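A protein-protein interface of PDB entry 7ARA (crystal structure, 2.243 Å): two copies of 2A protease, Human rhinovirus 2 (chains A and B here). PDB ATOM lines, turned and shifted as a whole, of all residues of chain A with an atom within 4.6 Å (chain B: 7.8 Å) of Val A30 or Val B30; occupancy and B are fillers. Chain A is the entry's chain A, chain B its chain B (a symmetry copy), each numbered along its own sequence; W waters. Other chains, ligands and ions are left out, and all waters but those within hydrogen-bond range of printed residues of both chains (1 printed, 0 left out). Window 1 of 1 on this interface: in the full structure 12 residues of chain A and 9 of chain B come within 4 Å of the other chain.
Val A30 touches two residues of chain B.
Of the printed residues of chain A, Val B30 touches Leu A29 (3.4 Å), Val A30 (2.7 Å) and Tyr A32 (3.6 Å).
Of the printed residues of chain B, Tyr A32 touches Met B24 (3.8 Å), Val B30 (3.6 Å) and Tyr B32 (2.2 Å).
Printed residues of chain A within 4 Å of Met B24: Tyr A32 (3.8 Å).
Of the printed residues of chain B, Ser A31 touches Leu B29.
Of the printed residues of chain B, Met A24 touches Tyr B32.
Printed residues of chain A within 4 Å of Leu B29: Val A30 (3.4 Å) and Ser A31 (3.7 Å).
The nearest residue of chain B that does not touch Val A30 is Ile B28 (4.04 Å).
The nearest printed residue of chain A that does not touch Val B30 is Ser A27 (5.0 Å).
The nearest printed residue of chain B that does not touch Ser A31 is Ile B28 (4.1 Å).
Printed residues of chain A that touch a printed residue of chain B: Met A24, Ser A27, Leu A29, Val A30, Ser A31 and Tyr A32.
Among the printed residues, 10 pairs touch across the chains.
Among the printed residues, no Asp or Glu carboxylate lies within 4 Å of a Lys or Arg side-chain nitrogen of the other chain.
The backbone carbonyl oxygen of Met A24 sits at hydrogen-bond distance from the side-chain hydroxyl of Ser A27 (2.7 Å).
O of Leu A36 is in hydrogen-bond range of N of Ser A31.
The backbone carbonyl oxygen of Ile B38 sits at hydrogen-bond distance from the backbone NH of Leu B29.
N of Ser B33 lies within hydrogen-bond range of O of Ser A27, at 3.1 Å.
O of Val B30 lies within hydrogen-bond range of N of Val A30.
The side-chain hydroxyl of Tyr A32 lies close to the side-chain hydroxyl of Tyr B32, 2.2 Å away.
Ser A27 touches Tyr B32, but with the chains exchanged Tyr A32 does not touch Ser B27 (7.4 Å).
Leu A29 touches Val B30, and with the chains exchanged Val A30 touches Leu B29.
Tyr A32 touches Val B30, but with the chains exchanged Val A30 does not touch Tyr B32 (4.2 Å).
Tyr B32 touches its own counterpart, Tyr A32.
9 positions are printed for both chains.
Of the 10 pairs that touch across the chains among the printed residues, 6 have their exchanged pair printed and touching as well.
Met A24 touches Tyr B32.
O of Ser A27 touches N of Tyr B32, at 3.9 Å.
O of Val B30 touches C of Leu A29 (3.4 Å).
Val A30 touches Leu B29.
Ser A31 touches Leu B29.
Met B24 touches Tyr A32 (CE to CB, 3.8 Å).
CE2 of Tyr A32 touches CG2 of Val B30, at 3.6 Å.
Water W1 bridges the backbone carbonyl oxygen (O) of Ile B28 (2.7 Å) and the backbone NH (N) of Tyr A32 (3.2 Å).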
ATOM      1  N   LEU A  17     -17.856  28.677 -12.008  1.00  0.00           N
ATOM      2  CA  LEU A  17     -17.876  27.869 -10.800  1.00  0.00           C
ATOM      3  C   LEU A  17     -16.519  27.232 -10.505  1.00  0.00           C
ATOM      4  O   LEU A  17     -16.093  27.181  -9.352  1.00  0.00           O
ATOM      5  CB  LEU A  17     -18.950  26.787 -10.903  1.00  0.00           C
ATOM      6  CG  LEU A  17     -18.986  25.792  -9.743  1.00  0.00           C
ATOM      7  CD1 LEU A  17     -19.266  26.510  -8.426  1.00  0.00           C
ATOM      8  CD2 LEU A  17     -20.024  24.717 -10.006  1.00  0.00           C
ATOM      9  N   MET A  24     -17.828  28.959  -1.911  1.00  0.00           N
ATOM     10  CA  MET A  24     -19.049  28.406  -2.491  1.00  0.00           C
ATOM     11  C   MET A  24     -20.238  28.413  -1.527  1.00  0.00           C
ATOM     12  O   MET A  24     -21.348  28.767  -1.917  1.00  0.00           O
ATOM     13  CB  MET A  24     -18.792  26.980  -2.987  1.00  0.00           C
ATOM     14  CG  MET A  24     -19.950  26.385  -3.778  1.00  0.00           C
ATOM     15  SD  MET A  24     -19.841  24.603  -4.056  1.00  0.00           S
ATOM     16  CE  MET A  24     -18.155  24.438  -4.624  1.00  0.00           C
ATOM     17  N   SER A  27     -22.263  31.500  -1.476  1.00  0.00           N
ATOM     18  CA  SER A  27     -22.867  31.916  -2.739  1.00  0.00           C
ATOM     19  C   SER A  27     -24.378  31.859  -2.652  1.00  0.00           C
ATOM     20  O   SER A  27     -24.927  31.144  -1.820  1.00  0.00           O
ATOM     21  CB  SER A  27     -22.400  31.023  -3.882  1.00  0.00           C
ATOM     22  OG  SER A  27     -23.026  29.756  -3.785  1.00  0.00           O
ATOM     23  N   LEU A  29     -26.267  31.111  -5.419  1.00  0.00           N
ATOM     24  CA  LEU A  29     -26.714  30.150  -6.433  1.00  0.00           C
ATOM     25  C   LEU A  29     -25.552  29.382  -7.066  1.00  0.00           C
ATOM     26  O   LEU A  29     -24.490  29.943  -7.317  1.00  0.00           O
ATOM     27  CB  LEU A  29     -27.514  30.854  -7.533  1.00  0.00           C
ATOM     28  CG  LEU A  29     -28.390  29.915  -8.367  1.00  0.00           C
ATOM     29  CD1 LEU A  29     -29.362  29.180  -7.464  1.00  0.00           C
ATOM     30  CD2 LEU A  29     -29.140  30.663  -9.451  1.00  0.00           C
ATOM     31  N   VAL A  30     -25.767  28.095  -7.325  1.00  0.00           N
ATOM     32  CA  VAL A  30     -24.747  27.232  -7.916  1.00  0.00           C
ATOM     33  C   VAL A  30     -25.361  26.226  -8.889  1.00  0.00           C
ATOM     34  O   VAL A  30     -26.366  25.585  -8.580  1.00  0.00           O
ATOM     35  CB  VAL A  30     -23.959  26.453  -6.831  1.00  0.00           C
ATOM     36  CG1 VAL A  30     -23.195  25.286  -7.446  1.00  0.00           C
ATOM     37  CG2 VAL A  30     -23.009  27.377  -6.083  1.00  0.00           C
ATOM     38  N   SER A  31     -24.753  26.097 -10.063  1.00  0.00           N
ATOM     39  CA  SER A  31     -25.140  25.077 -11.032  1.00  0.00           C
ATOM     40  C   SER A  31     -23.933  24.234 -11.430  1.00  0.00           C
ATOM     41  O   SER A  31     -23.167  24.623 -12.310  1.00  0.00           O
ATOM     42  CB  SER A  31     -25.764  25.719 -12.271  1.00  0.00           C
ATOM     43  OG  SER A  31     -26.010  24.754 -13.277  1.00  0.00           O
ATOM     44  N   TYR A  32     -23.771  23.079 -10.787  1.00  0.00           N
ATOM     45  CA  TYR A  32     -22.599  22.228 -11.002  1.00  0.00           C
ATOM     46  C   TYR A  32     -22.486  21.750 -12.438  1.00  0.00           C
ATOM     47  O   TYR A  32     -21.383  21.529 -12.940  1.00  0.00           O
ATOM     48  CB  TYR A  32     -22.635  21.017 -10.070  1.00  0.00           C
ATOM     49  CG  TYR A  32     -22.792  21.370  -8.610  1.00  0.00           C
ATOM     50  CD1 TYR A  32     -21.710  21.829  -7.866  1.00  0.00           C
ATOM     51  CD2 TYR A  32     -24.018  21.239  -7.973  1.00  0.00           C
ATOM     52  CE1 TYR A  32     -21.848  22.152  -6.531  1.00  0.00           C
ATOM     53  CE2 TYR A  32     -24.165  21.557  -6.640  1.00  0.00           C
ATOM     54  CZ  TYR A  32     -23.077  22.015  -5.924  1.00  0.00           C
ATOM     55  OH  TYR A  32     -23.221  22.333  -4.593  1.00  0.00           O
ATOM     56  N   LEU A  36     -21.693  27.460 -13.342  1.00  0.00           N
ATOM     57  CA  LEU A  36     -22.092  28.805 -12.949  1.00  0.00           C
ATOM     58  C   LEU A  36     -22.125  28.963 -11.438  1.00  0.00           C
ATOM     59  O   LEU A  36     -22.396  28.007 -10.713  1.00  0.00           O
ATOM     60  CB  LEU A  36     -23.464  29.146 -13.525  1.00  0.00           C
ATOM     61  CG  LEU A  36     -23.942  30.569 -13.226  1.00  0.00           C
ATOM     62  CD1 LEU A  36     -23.024  31.585 -13.890  1.00  0.00           C
ATOM     63  CD2 LEU A  36     -25.388  30.778 -13.646  1.00  0.00           C
ATOM     64  N   ILE A  37     -21.847  30.175 -10.969  1.00  0.00           N
ATOM     65  CA  ILE A  37     -22.011  30.498  -9.561  1.00  0.00           C
ATOM     66  C   ILE A  37     -22.351  31.981  -9.417  1.00  0.00           C
ATOM     67  O   ILE A  37     -21.907  32.808 -10.209  1.00  0.00           O
ATOM     68  CB  ILE A  37     -20.747  30.139  -8.758  1.00  0.00           C
ATOM     69  CG1 ILE A  37     -21.006  30.262  -7.258  1.00  0.00           C
ATOM     70  CG2 ILE A  37     -19.567  30.994  -9.195  1.00  0.00           C
ATOM     71  CD1 ILE A  37     -19.948  29.604  -6.416  1.00  0.00           C
ATOM     72  N   LEU B  17     -32.057  22.059   1.515  1.00  0.00           N
ATOM     73  CA  LEU B  17     -30.778  21.561   1.047  1.00  0.00           C
ATOM     74  C   LEU B  17     -30.304  20.353   1.854  1.00  0.00           C
ATOM     75  O   LEU B  17     -29.886  19.348   1.279  1.00  0.00           O
ATOM     76  CB  LEU B  17     -29.734  22.674   1.097  1.00  0.00           C
ATOM     77  CG  LEU B  17     -28.391  22.314   0.471  1.00  0.00           C
ATOM     78  CD1 LEU B  17     -28.581  21.912  -0.986  1.00  0.00           C
ATOM     79  CD2 LEU B  17     -27.435  23.481   0.601  1.00  0.00           C
ATOM     80  N   PHE B  20     -31.401  16.651   1.375  1.00  0.00           N
ATOM     81  CA  PHE B  20     -31.001  15.994   0.141  1.00  0.00           C
ATOM     82  C   PHE B  20     -29.994  14.878   0.410  1.00  0.00           C
ATOM     83  O   PHE B  20     -29.032  15.049   1.166  1.00  0.00           O
ATOM     84  CB  PHE B  20     -30.422  17.010  -0.843  1.00  0.00           C
ATOM     85  CG  PHE B  20     -30.294  16.489  -2.248  1.00  0.00           C
ATOM     86  CD1 PHE B  20     -31.413  16.369  -3.059  1.00  0.00           C
ATOM     87  CD2 PHE B  20     -29.056  16.128  -2.761  1.00  0.00           C
ATOM     88  CE1 PHE B  20     -31.300  15.891  -4.356  1.00  0.00           C
ATOM     89  CE2 PHE B  20     -28.934  15.650  -4.055  1.00  0.00           C
ATOM     90  CZ  PHE B  20     -30.058  15.533  -4.853  1.00  0.00           C
ATOM     91  N   MET B  24     -27.070  12.885  -8.163  1.00  0.00           N
ATOM     92  CA  MET B  24     -26.672  14.100  -8.864  1.00  0.00           C
ATOM     93  C   MET B  24     -27.339  14.152 -10.238  1.00  0.00           C
ATOM     94  O   MET B  24     -27.331  13.170 -10.980  1.00  0.00           O
ATOM     95  CB  MET B  24     -25.145  14.167  -9.005  1.00  0.00           C
ATOM     96  CG  MET B  24     -24.653  15.228  -9.987  1.00  0.00           C
ATOM     97  SD  MET B  24     -25.129  16.910  -9.525  1.00  0.00           S
ATOM     98  CE  MET B  24     -24.538  17.849 -10.934  1.00  0.00           C
ATOM     99  N   SER B  27     -30.010  19.093 -13.751  1.00  0.00           N
ATOM    100  CA  SER B  27     -30.865  20.245 -13.476  1.00  0.00           C
ATOM    101  C   SER B  27     -30.727  20.787 -12.052  1.00  0.00           C
ATOM    102  O   SER B  27     -31.364  21.782 -11.698  1.00  0.00           O
ATOM    103  CB  SER B  27     -32.330  19.888 -13.754  1.00  0.00           C
ATOM    104  OG  SER B  27     -32.781  18.835 -12.919  1.00  0.00           O
ATOM    105  N   ILE B  28     -29.888  20.146 -11.242  1.00  0.00           N
ATOM    106  CA  ILE B  28     -29.706  20.566  -9.856  1.00  0.00           C
ATOM    107  C   ILE B  28     -29.146  21.990  -9.726  1.00  0.00           C
ATOM    108  O   ILE B  28     -28.045  22.288 -10.199  1.00  0.00           O
ATOM    109  CB  ILE B  28     -28.780  19.602  -9.099  1.00  0.00           C
ATOM    110  CG1 ILE B  28     -29.470  18.254  -8.908  1.00  0.00           C
ATOM    111  CG2 ILE B  28     -28.395  20.181  -7.745  1.00  0.00           C
ATOM    112  CD1 ILE B  28     -28.699  17.285  -8.035  1.00  0.00           C
ATOM    113  N   LEU B  29     -29.931  22.859  -9.092  1.00  0.00           N
ATOM    114  CA  LEU B  29     -29.494  24.192  -8.687  1.00  0.00           C
ATOM    115  C   LEU B  29     -29.383  24.245  -7.172  1.00  0.00           C
ATOM    116  O   LEU B  29     -30.250  23.718  -6.472  1.00  0.00           O
ATOM    117  CB  LEU B  29     -30.476  25.265  -9.165  1.00  0.00           C
ATOM    118  CG  LEU B  29     -30.643  25.475 -10.667  1.00  0.00           C
ATOM    119  CD1 LEU B  29     -31.595  26.627 -10.929  1.00  0.00           C
ATOM    120  CD2 LEU B  29     -29.299  25.738 -11.307  1.00  0.00           C
ATOM    121  N   VAL B  30     -28.335  24.877  -6.651  1.00  0.00           N
ATOM    122  CA  VAL B  30     -28.187  24.957  -5.202  1.00  0.00           C
ATOM    123  C   VAL B  30     -27.940  26.367  -4.695  1.00  0.00           C
ATOM    124  O   VAL B  30     -27.021  27.052  -5.147  1.00  0.00           O
ATOM    125  CB  VAL B  30     -27.039  24.078  -4.692  1.00  0.00           C
ATOM    126  CG1 VAL B  30     -26.934  24.199  -3.181  1.00  0.00           C
ATOM    127  CG2 VAL B  30     -27.257  22.635  -5.097  1.00  0.00           C
ATOM    128  N   SER B  31     -28.760  26.789  -3.740  1.00  0.00           N
ATOM    129  CA  SER B  31     -28.540  28.057  -3.064  1.00  0.00           C
ATOM    130  C   SER B  31     -28.071  27.822  -1.637  1.00  0.00           C
ATOM    131  O   SER B  31     -28.882  27.687  -0.721  1.00  0.00           O
ATOM    132  CB  SER B  31     -29.810  28.903  -3.066  1.00  0.00           C
ATOM    133  OG  SER B  31     -29.588  30.140  -2.414  1.00  0.00           O
ATOM    134  N   TYR B  32     -26.755  27.772  -1.456  1.00  0.00           N
ATOM    135  CA  TYR B  32     -26.174  27.564  -0.136  1.00  0.00           C
ATOM    136  C   TYR B  32     -26.596  28.649   0.848  1.00  0.00           C
ATOM    137  O   TYR B  32     -26.779  28.388   2.037  1.00  0.00           O
ATOM    138  CB  TYR B  32     -24.653  27.498  -0.237  1.00  0.00           C
ATOM    139  CG  TYR B  32     -24.170  26.197  -0.825  1.00  0.00           C
ATOM    140  CD1 TYR B  32     -24.045  25.068  -0.029  1.00  0.00           C
ATOM    141  CD2 TYR B  32     -23.844  26.094  -2.171  1.00  0.00           C
ATOM    142  CE1 TYR B  32     -23.611  23.869  -0.553  1.00  0.00           C
ATOM    143  CE2 TYR B  32     -23.403  24.896  -2.707  1.00  0.00           C
ATOM    144  CZ  TYR B  32     -23.292  23.787  -1.889  1.00  0.00           C
ATOM    145  OH  TYR B  32     -22.857  22.588  -2.402  1.00  0.00           O
ATOM    146  N   SER B  33     -26.769  29.864   0.341  1.00  0.00           N
ATOM    147  CA  SER B  33     -27.205  30.985   1.163  1.00  0.00           C
ATOM    148  C   SER B  33     -28.706  30.997   1.459  1.00  0.00           C
ATOM    149  O   SER B  33     -29.221  31.987   1.975  1.00  0.00           O
ATOM    150  CB  SER B  33     -26.825  32.299   0.488  1.00  0.00           C
ATOM    151  OG  SER B  33     -27.777  33.303   0.791  1.00  0.00           O
ATOM    152  N   SER B  34     -29.412  29.918   1.131  1.00  0.00           N
ATOM    153  CA  SER B  34     -30.852  29.861   1.375  1.00  0.00           C
ATOM    154  C   SER B  34     -31.312  28.470   1.790  1.00  0.00           C
ATOM    155  O   SER B  34     -32.509  28.251   1.979  1.00  0.00           O
ATOM    156  CB  SER B  34     -31.632  30.300   0.131  1.00  0.00           C
ATOM    157  OG  SER B  34     -31.264  31.606  -0.280  1.00  0.00           O
ATOM    158  N   ASP B  35     -30.362  27.544   1.926  1.00  0.00           N
ATOM    159  CA  ASP B  35     -30.661  26.161   2.306  1.00  0.00           C
ATOM    160  C   ASP B  35     -31.702  25.564   1.357  1.00  0.00           C
ATOM    161  O   ASP B  35     -32.688  24.959   1.784  1.00  0.00           O
ATOM    162  CB  ASP B  35     -31.146  26.097   3.759  1.00  0.00           C
ATOM    163  CG  ASP B  35     -31.291  24.675   4.273  1.00  0.00           C
ATOM    164  OD1 ASP B  35     -30.412  23.835   3.978  1.00  0.00           O
ATOM    165  OD2 ASP B  35     -32.298  24.405   4.967  1.00  0.00           O
ATOM    166  N   LEU B  36     -31.479  25.750   0.061  1.00  0.00           N
ATOM    167  CA  LEU B  36     -32.449  25.338  -0.946  1.00  0.00           C
ATOM    168  C   LEU B  36     -31.787  24.605  -2.099  1.00  0.00           C
ATOM    169  O   LEU B  36     -30.738  25.020  -2.590  1.00  0.00           O
ATOM    170  CB  LEU B  36     -33.211  26.551  -1.484  1.00  0.00           C
ATOM    171  CG  LEU B  36     -34.336  26.244  -2.474  1.00  0.00           C
ATOM    172  CD1 LEU B  36     -35.555  25.760  -1.731  1.00  0.00           C
ATOM    173  CD2 LEU B  36     -34.680  27.452  -3.335  1.00  0.00           C
ATOM    174  N   ILE B  37     -32.399  23.510  -2.529  1.00  0.00           N
ATOM    175  CA  ILE B  37     -31.954  22.844  -3.737  1.00  0.00           C
ATOM    176  C   ILE B  37     -33.144  22.713  -4.676  1.00  0.00           C
ATOM    177  O   ILE B  37     -34.267  22.464  -4.243  1.00  0.00           O
ATOM    178  CB  ILE B  37     -31.327  21.461  -3.436  1.00  0.00           C
ATOM    179  CG1 ILE B  37     -30.767  20.834  -4.716  1.00  0.00           C
ATOM    180  CG2 ILE B  37     -32.331  20.541  -2.763  1.00  0.00           C
ATOM    181  CD1 ILE B  37     -30.061  19.522  -4.486  1.00  0.00           C
ATOM    182  N   ILE B  38     -32.897  22.928  -5.961  1.00  0.00           N
ATOM    183  CA  ILE B  38     -33.936  22.802  -6.972  1.00  0.00           C
ATOM    184  C   ILE B  38     -33.495  21.813  -8.037  1.00  0.00           C
ATOM    185  O   ILE B  38     -32.367  21.886  -8.519  1.00  0.00           O
ATOM    186  CB  ILE B  38     -34.249  24.151  -7.642  1.00  0.00           C
ATOM    187  CG1 ILE B  38     -34.520  25.232  -6.597  1.00  0.00           C
ATOM    188  CG2 ILE B  38     -35.430  24.016  -8.587  1.00  0.00           C
ATOM    189  CD1 ILE B  38     -34.602  26.625  -7.191  1.00  0.00           C
ATOM    190  N   TYR B  39     -34.375  20.890  -8.407  1.00  0.00           N
ATOM    191  CA  TYR B  39     -34.056  19.935  -9.462  1.00  0.00           C
ATOM    192  C   TYR B  39     -35.309  19.421 -10.164  1.00  0.00           C
ATOM    193  O   TYR B  39     -36.420  19.584  -9.661  1.00  0.00           O
ATOM    194  CB  TYR B  39     -33.254  18.766  -8.894  1.00  0.00           C
ATOM    195  CG  TYR B  39     -33.943  18.028  -7.769  1.00  0.00           C
ATOM    196  CD1 TYR B  39     -34.784  16.953  -8.029  1.00  0.00           C
ATOM    197  CD2 TYR B  39     -33.740  18.395  -6.444  1.00  0.00           C
ATOM    198  CE1 TYR B  39     -35.411  16.268  -6.999  1.00  0.00           C
ATOM    199  CE2 TYR B  39     -34.362  17.715  -5.408  1.00  0.00           C
ATOM    200  CZ  TYR B  39     -35.195  16.655  -5.692  1.00  0.00           C
ATOM    201  OH  TYR B  39     -35.814  15.979  -4.667  1.00  0.00           O
ATOM    202  N   PHE B 136     -37.179  32.431  -6.386  1.00  0.00           N
ATOM    203  CA  PHE B 136     -36.512  31.416  -7.198  1.00  0.00           C
ATOM    204  C   PHE B 136     -37.427  30.853  -8.292  1.00  0.00           C
ATOM    205  O   PHE B 136     -37.221  29.734  -8.763  1.00  0.00           O
ATOM    206  CB  PHE B 136     -36.021  30.262  -6.320  1.00  0.00           C
ATOM    207  CG  PHE B 136     -35.071  30.675  -5.226  1.00  0.00           C
ATOM    208  CD1 PHE B 136     -35.549  31.041  -3.979  1.00  0.00           C
ATOM    209  CD2 PHE B 136     -33.702  30.656  -5.433  1.00  0.00           C
ATOM    210  CE1 PHE B 136     -34.679  31.404  -2.966  1.00  0.00           C
ATOM    211  CE2 PHE B 136     -32.823  31.017  -4.421  1.00  0.00           C
ATOM    212  CZ  PHE B 136     -33.312  31.391  -3.188  1.00  0.00           C
HETATM  213  O   HOH W   1     -26.174  21.254 -11.774  1.00  0.00           O
